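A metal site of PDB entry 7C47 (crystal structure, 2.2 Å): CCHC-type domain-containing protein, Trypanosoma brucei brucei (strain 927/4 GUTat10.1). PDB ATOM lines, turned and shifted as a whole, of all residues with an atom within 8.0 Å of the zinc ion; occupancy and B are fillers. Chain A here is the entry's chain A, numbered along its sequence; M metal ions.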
ATOM      1  N   LYS A 280     -12.559 -23.995  -7.796  1.00  0.00           N
ATOM      2  CA  LYS A 280     -11.468 -24.272  -6.870  1.00  0.00           C
ATOM      3  C   LYS A 280     -10.820 -25.583  -7.301  1.00  0.00           C
ATOM      4  O   LYS A 280     -11.505 -26.605  -7.429  1.00  0.00           O
ATOM      5  CB  LYS A 280     -12.008 -24.393  -5.445  1.00  0.00           C
ATOM      6  CG  LYS A 280     -10.953 -24.514  -4.368  1.00  0.00           C
ATOM      7  CD  LYS A 280     -11.584 -24.577  -2.978  1.00  0.00           C
ATOM      8  CE  LYS A 280     -10.547 -24.869  -1.902  1.00  0.00           C
ATOM      9  NZ  LYS A 280      -9.454 -23.864  -1.883  1.00  0.00           N
ATOM     10  N   CYS A 281      -9.504 -25.566  -7.528  1.00  0.00           N
ATOM     11  CA  CYS A 281      -8.803 -26.719  -8.068  1.00  0.00           C
ATOM     12  C   CYS A 281      -8.661 -27.826  -7.030  1.00  0.00           C
ATOM     13  O   CYS A 281      -8.012 -27.644  -6.004  1.00  0.00           O
ATOM     14  CB  CYS A 281      -7.411 -26.325  -8.570  1.00  0.00           C
ATOM     15  SG  CYS A 281      -6.526 -27.717  -9.282  1.00  0.00           S
ATOM     16  N   SER A 282      -9.255 -28.984  -7.327  1.00  0.00           N
ATOM     17  CA  SER A 282      -9.244 -30.124  -6.397  1.00  0.00           C
ATOM     18  C   SER A 282      -7.843 -30.712  -6.188  1.00  0.00           C
ATOM     19  O   SER A 282      -7.593 -31.318  -5.153  1.00  0.00           O
ATOM     20  CB  SER A 282     -10.230 -31.212  -6.857  1.00  0.00           C
ATOM     21  OG  SER A 282      -9.888 -31.730  -8.125  1.00  0.00           O
ATOM     22  N   PHE A 283      -6.944 -30.525  -7.156  1.00  0.00           N
ATOM     23  CA  PHE A 283      -5.580 -31.040  -7.061  1.00  0.00           C
ATOM     24  C   PHE A 283      -4.614 -30.110  -6.318  1.00  0.00           C
ATOM     25  O   PHE A 283      -3.869 -30.582  -5.456  1.00  0.00           O
ATOM     26  CB  PHE A 283      -5.024 -31.344  -8.458  1.00  0.00           C
ATOM     27  CG  PHE A 283      -3.714 -32.090  -8.437  1.00  0.00           C
ATOM     28  CD1 PHE A 283      -3.674 -33.439  -8.107  1.00  0.00           C
ATOM     29  CD2 PHE A 283      -2.513 -31.437  -8.742  1.00  0.00           C
ATOM     30  CE1 PHE A 283      -2.476 -34.130  -8.080  1.00  0.00           C
ATOM     31  CE2 PHE A 283      -1.310 -32.133  -8.723  1.00  0.00           C
ATOM     32  CZ  PHE A 283      -1.295 -33.477  -8.395  1.00  0.00           C
ATOM     33  N   CYS A 284      -4.604 -28.823  -6.668  1.00  0.00           N
ATOM     34  CA  CYS A 284      -3.653 -27.852  -6.073  1.00  0.00           C
ATOM     35  C   CYS A 284      -4.267 -26.838  -5.099  1.00  0.00           C
ATOM     36  O   CYS A 284      -3.528 -26.082  -4.469  1.00  0.00           O
ATOM     37  CB  CYS A 284      -2.890 -27.120  -7.183  1.00  0.00           C
ATOM     38  SG  CYS A 284      -3.811 -25.810  -8.032  1.00  0.00           S
ATOM     39  N   GLY A 285      -5.598 -26.798  -4.991  1.00  0.00           N
ATOM     40  CA  GLY A 285      -6.284 -25.942  -4.013  1.00  0.00           C
ATOM     41  C   GLY A 285      -6.562 -24.495  -4.408  1.00  0.00           C
ATOM     42  O   GLY A 285      -7.314 -23.815  -3.717  1.00  0.00           O
ATOM     43  N   GLU A 286      -5.995 -24.019  -5.518  1.00  0.00           N
ATOM     44  CA  GLU A 286      -6.095 -22.611  -5.904  1.00  0.00           C
ATOM     45  C   GLU A 286      -7.461 -22.282  -6.506  1.00  0.00           C
ATOM     46  O   GLU A 286      -8.009 -23.069  -7.281  1.00  0.00           O
ATOM     47  CB  GLU A 286      -5.016 -22.236  -6.923  1.00  0.00           C
ATOM     48  CG  GLU A 286      -3.579 -22.383  -6.434  1.00  0.00           C
ATOM     49  CD  GLU A 286      -2.552 -22.169  -7.546  1.00  0.00           C
ATOM     50  OE1 GLU A 286      -2.908 -21.578  -8.602  1.00  0.00           O
ATOM     51  OE2 GLU A 286      -1.392 -22.578  -7.358  1.00  0.00           O
ATOM     52  N   VAL A 287      -7.992 -21.114  -6.156  1.00  0.00           N
ATOM     53  CA  VAL A 287      -9.231 -20.603  -6.744  1.00  0.00           C
ATOM     54  C   VAL A 287      -8.900 -20.047  -8.138  1.00  0.00           C
ATOM     55  O   VAL A 287      -7.836 -19.469  -8.342  1.00  0.00           O
ATOM     56  CB  VAL A 287      -9.882 -19.500  -5.854  1.00  0.00           C
ATOM     57  CG1 VAL A 287     -11.114 -18.894  -6.521  1.00  0.00           C
ATOM     58  CG2 VAL A 287     -10.237 -20.067  -4.491  1.00  0.00           C
ATOM     59  N   HIS A 289      -9.311 -21.994 -11.307  1.00  0.00           N
ATOM     60  CA  HIS A 289      -9.369 -23.078 -12.297  1.00  0.00           C
ATOM     61  C   HIS A 289      -9.717 -24.422 -11.662  1.00  0.00           C
ATOM     62  O   HIS A 289      -9.650 -24.581 -10.455  1.00  0.00           O
ATOM     63  CB  HIS A 289      -8.049 -23.195 -13.050  1.00  0.00           C
ATOM     64  CG  HIS A 289      -6.876 -23.524 -12.180  1.00  0.00           C
ATOM     65  ND1 HIS A 289      -6.314 -22.601 -11.317  1.00  0.00           N
ATOM     66  CD2 HIS A 289      -6.154 -24.663 -12.029  1.00  0.00           C
ATOM     67  CE1 HIS A 289      -5.295 -23.160 -10.680  1.00  0.00           C
ATOM     68  NE2 HIS A 289      -5.187 -24.408 -11.088  1.00  0.00           N
ATOM     69  N   THR A 290     -10.092 -25.389 -12.511  1.00  0.00           N
ATOM     70  CA  THR A 290     -10.424 -26.744 -12.068  1.00  0.00           C
ATOM     71  C   THR A 290      -9.249 -27.677 -12.325  1.00  0.00           C
ATOM     72  O   THR A 290      -8.301 -27.330 -13.031  1.00  0.00           O
ATOM     73  CB  THR A 290     -11.687 -27.276 -12.768  1.00  0.00           C
ATOM     74  OG1 THR A 290     -11.451 -27.381 -14.174  1.00  0.00           O
ATOM     75  CG2 THR A 290     -12.863 -26.355 -12.517  1.00  0.00           C
ATOM     76  N   ALA A 291      -9.325 -28.876 -11.747  1.00  0.00           N
ATOM     77  CA  ALA A 291      -8.229 -29.854 -11.829  1.00  0.00           C
ATOM     78  C   ALA A 291      -7.942 -30.305 -13.264  1.00  0.00           C
ATOM     79  O   ALA A 291      -6.795 -30.578 -13.605  1.00  0.00           O
ATOM     80  CB  ALA A 291      -8.501 -31.058 -10.945  1.00  0.00           C
ATOM     81  N   ARG A 292      -8.977 -30.362 -14.089  1.00  0.00           N
ATOM     82  CA  ARG A 292      -8.833 -30.747 -15.504  1.00  0.00           C
ATOM     83  C   ARG A 292      -7.988 -29.751 -16.313  1.00  0.00           C
ATOM     84  O   ARG A 292      -7.395 -30.140 -17.315  1.00  0.00           O
ATOM     85  CB  ARG A 292     -10.206 -30.973 -16.148  1.00  0.00           C
ATOM     86  CG  ARG A 292     -11.008 -32.077 -15.461  1.00  0.00           C
ATOM     87  CD  ARG A 292     -11.595 -33.107 -16.430  1.00  0.00           C
ATOM     88  NE  ARG A 292     -12.819 -32.653 -17.082  1.00  0.00           N
ATOM     89  CZ  ARG A 292     -13.422 -33.273 -18.109  1.00  0.00           C
ATOM     90  NH1 ARG A 292     -14.542 -32.761 -18.616  1.00  0.00           N
ATOM     91  NH2 ARG A 292     -12.914 -34.400 -18.634  1.00  0.00           N
ATOM     92  N   ASN A 293      -7.947 -28.493 -15.873  1.00  0.00           N
ATOM     93  CA  ASN A 293      -7.127 -27.440 -16.479  1.00  0.00           C
ATOM     94  C   ASN A 293      -5.879 -27.066 -15.664  1.00  0.00           C
ATOM     95  O   ASN A 293      -5.250 -26.045 -15.938  1.00  0.00           O
ATOM     96  CB  ASN A 293      -7.996 -26.192 -16.681  1.00  0.00           C
ATOM     97  CG  ASN A 293      -9.184 -26.458 -17.579  1.00  0.00           C
ATOM     98  OD1 ASN A 293      -9.043 -27.032 -18.665  1.00  0.00           O
ATOM     99  ND2 ASN A 293     -10.367 -26.049 -17.139  1.00  0.00           N
ATOM    100  N   CYS A 294      -5.493 -27.913 -14.703  1.00  0.00           N
ATOM    101  CA  CYS A 294      -4.384 -27.601 -13.792  1.00  0.00           C
ATOM    102  C   CYS A 294      -3.050 -27.983 -14.426  1.00  0.00           C
ATOM    103  O   CYS A 294      -2.877 -29.121 -14.868  1.00  0.00           O
ATOM    104  CB  CYS A 294      -4.563 -28.360 -12.482  1.00  0.00           C
ATOM    105  SG  CYS A 294      -3.369 -27.937 -11.196  1.00  0.00           S
ATOM    106  N   PHE A 295      -2.109 -27.049 -14.446  1.00  0.00           N
ATOM    107  CA  PHE A 295      -0.764 -27.290 -14.984  1.00  0.00           C
ATOM    108  C   PHE A 295       0.075 -28.217 -14.091  1.00  0.00           C
ATOM    109  O   PHE A 295       0.946 -28.920 -14.593  1.00  0.00           O
ATOM    110  CB  PHE A 295       0.020 -25.986 -15.183  1.00  0.00           C
ATOM    111  CG  PHE A 295      -0.631 -25.015 -16.139  1.00  0.00           C
ATOM    112  CD1 PHE A 295      -1.041 -25.422 -17.414  1.00  0.00           C
ATOM    113  CD2 PHE A 295      -0.793 -23.675 -15.788  1.00  0.00           C
ATOM    114  CE1 PHE A 295      -1.631 -24.523 -18.306  1.00  0.00           C
ATOM    115  CE2 PHE A 295      -1.387 -22.771 -16.672  1.00  0.00           C
ATOM    116  CZ  PHE A 295      -1.806 -23.195 -17.931  1.00  0.00           C
ATOM    117  N   LYS A 296      -0.166 -28.195 -12.781  1.00  0.00           N
ATOM    118  CA  LYS A 296       0.519 -29.109 -11.860  1.00  0.00           C
ATOM    119  C   LYS A 296       0.101 -30.556 -12.104  1.00  0.00           C
ATOM    120  O   LYS A 296       0.948 -31.440 -12.242  1.00  0.00           O
ATOM    121  CB  LYS A 296       0.246 -28.749 -10.388  1.00  0.00           C
ATOM    122  CG  LYS A 296       1.124 -27.645  -9.830  1.00  0.00           C
ATOM    123  CD  LYS A 296       0.616 -26.254 -10.190  1.00  0.00           C
ATOM    124  CE  LYS A 296       1.230 -25.190  -9.284  1.00  0.00           C
ATOM    125  NZ  LYS A 296       0.783 -25.304  -7.865  1.00  0.00           N
ATOM    126  N   LYS A 297      -1.208 -30.798 -12.154  1.00  0.00           N
ATOM    127  CA  LYS A 297      -1.754 -32.133 -12.416  1.00  0.00           C
ATOM    128  C   LYS A 297      -1.464 -32.634 -13.839  1.00  0.00           C
ATOM    129  O   LYS A 297      -1.197 -33.817 -14.020  1.00  0.00           O
ATOM    130  CB  LYS A 297      -3.262 -32.148 -12.175  1.00  0.00           C
ATOM    131  CG  LYS A 297      -3.865 -33.541 -12.245  1.00  0.00           C
ATOM    132  CD  LYS A 297      -5.228 -33.576 -11.573  1.00  0.00           C
ATOM    133  CE  LYS A 297      -5.793 -34.978 -11.608  1.00  0.00           C
ATOM    134  NZ  LYS A 297      -7.080 -35.036 -10.889  1.00  0.00           N
ATOM    135  N   HIS A 298      -1.526 -31.722 -14.807  1.00  0.00           N
ATOM    136  CA  HIS A 298      -1.372 -32.054 -16.230  1.00  0.00           C
ATOM    137  C   HIS A 298      -0.258 -31.196 -16.843  1.00  0.00           C
ATOM    138  O   HIS A 298      -0.539 -30.172 -17.475  1.00  0.00           O
ATOM    139  CB  HIS A 298      -2.705 -31.841 -16.965  1.00  0.00           C
ATOM    140  CG  HIS A 298      -3.871 -32.551 -16.350  1.00  0.00           C
ATOM    141  ND1 HIS A 298      -4.026 -33.924 -16.405  1.00  0.00           N
ATOM    142  CD2 HIS A 298      -4.949 -32.075 -15.685  1.00  0.00           C
ATOM    143  CE1 HIS A 298      -5.148 -34.259 -15.789  1.00  0.00           C
ATOM    144  NE2 HIS A 298      -5.723 -33.158 -15.344  1.00  0.00           N
HETATM  145 ZN    ZN M   1      -4.580 -26.698  -9.833  1.00  0.00          ZN
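The side-chain sulfur (SG) of Cys 284 lies close to a ring nitrogen (NE2) of His 289, at 3.6 Å. The side-chain sulfur (SG) of Cys 284 lies close to the backbone NH (N) of Glu 286 (3.8 Å). SG of Cys 294 lies close to N of Lys 296, at 3.6 Å. N of Lys 297 sits close to SG of Cys 294 (3.7 Å). The backbone NH (N) of Cys 281 lies within hydrogen-bond range of the backbone carbonyl oxygen (O) of His 289 (3.1 Å). The backbone NH (N) of Phe 283 sits close to the side-chain sulfur (SG) of Cys 281, at 3.5 Å. N of Cys 281 is in hydrogen-bond range of O of Glu 286 (2.9 Å).
Four residues have an atom within 4 Å of the zinc ion: Cys 281, Cys 284, His 289 and Cys 294. The nearest printed residue that does not touch the zinc ion is Phe 283 (4.9 Å).
The zinc ion is bound by the side-chain sulfur (SG) of Cys 284 (2.2 Å), the side-chain sulfur (SG) of Cys 294 (2.2 Å) and the side-chain sulfur (SG) of Cys 281 (2.3 Å). Slightly farther from the zinc ion lies NE2 of His 289 (2.7 Å).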
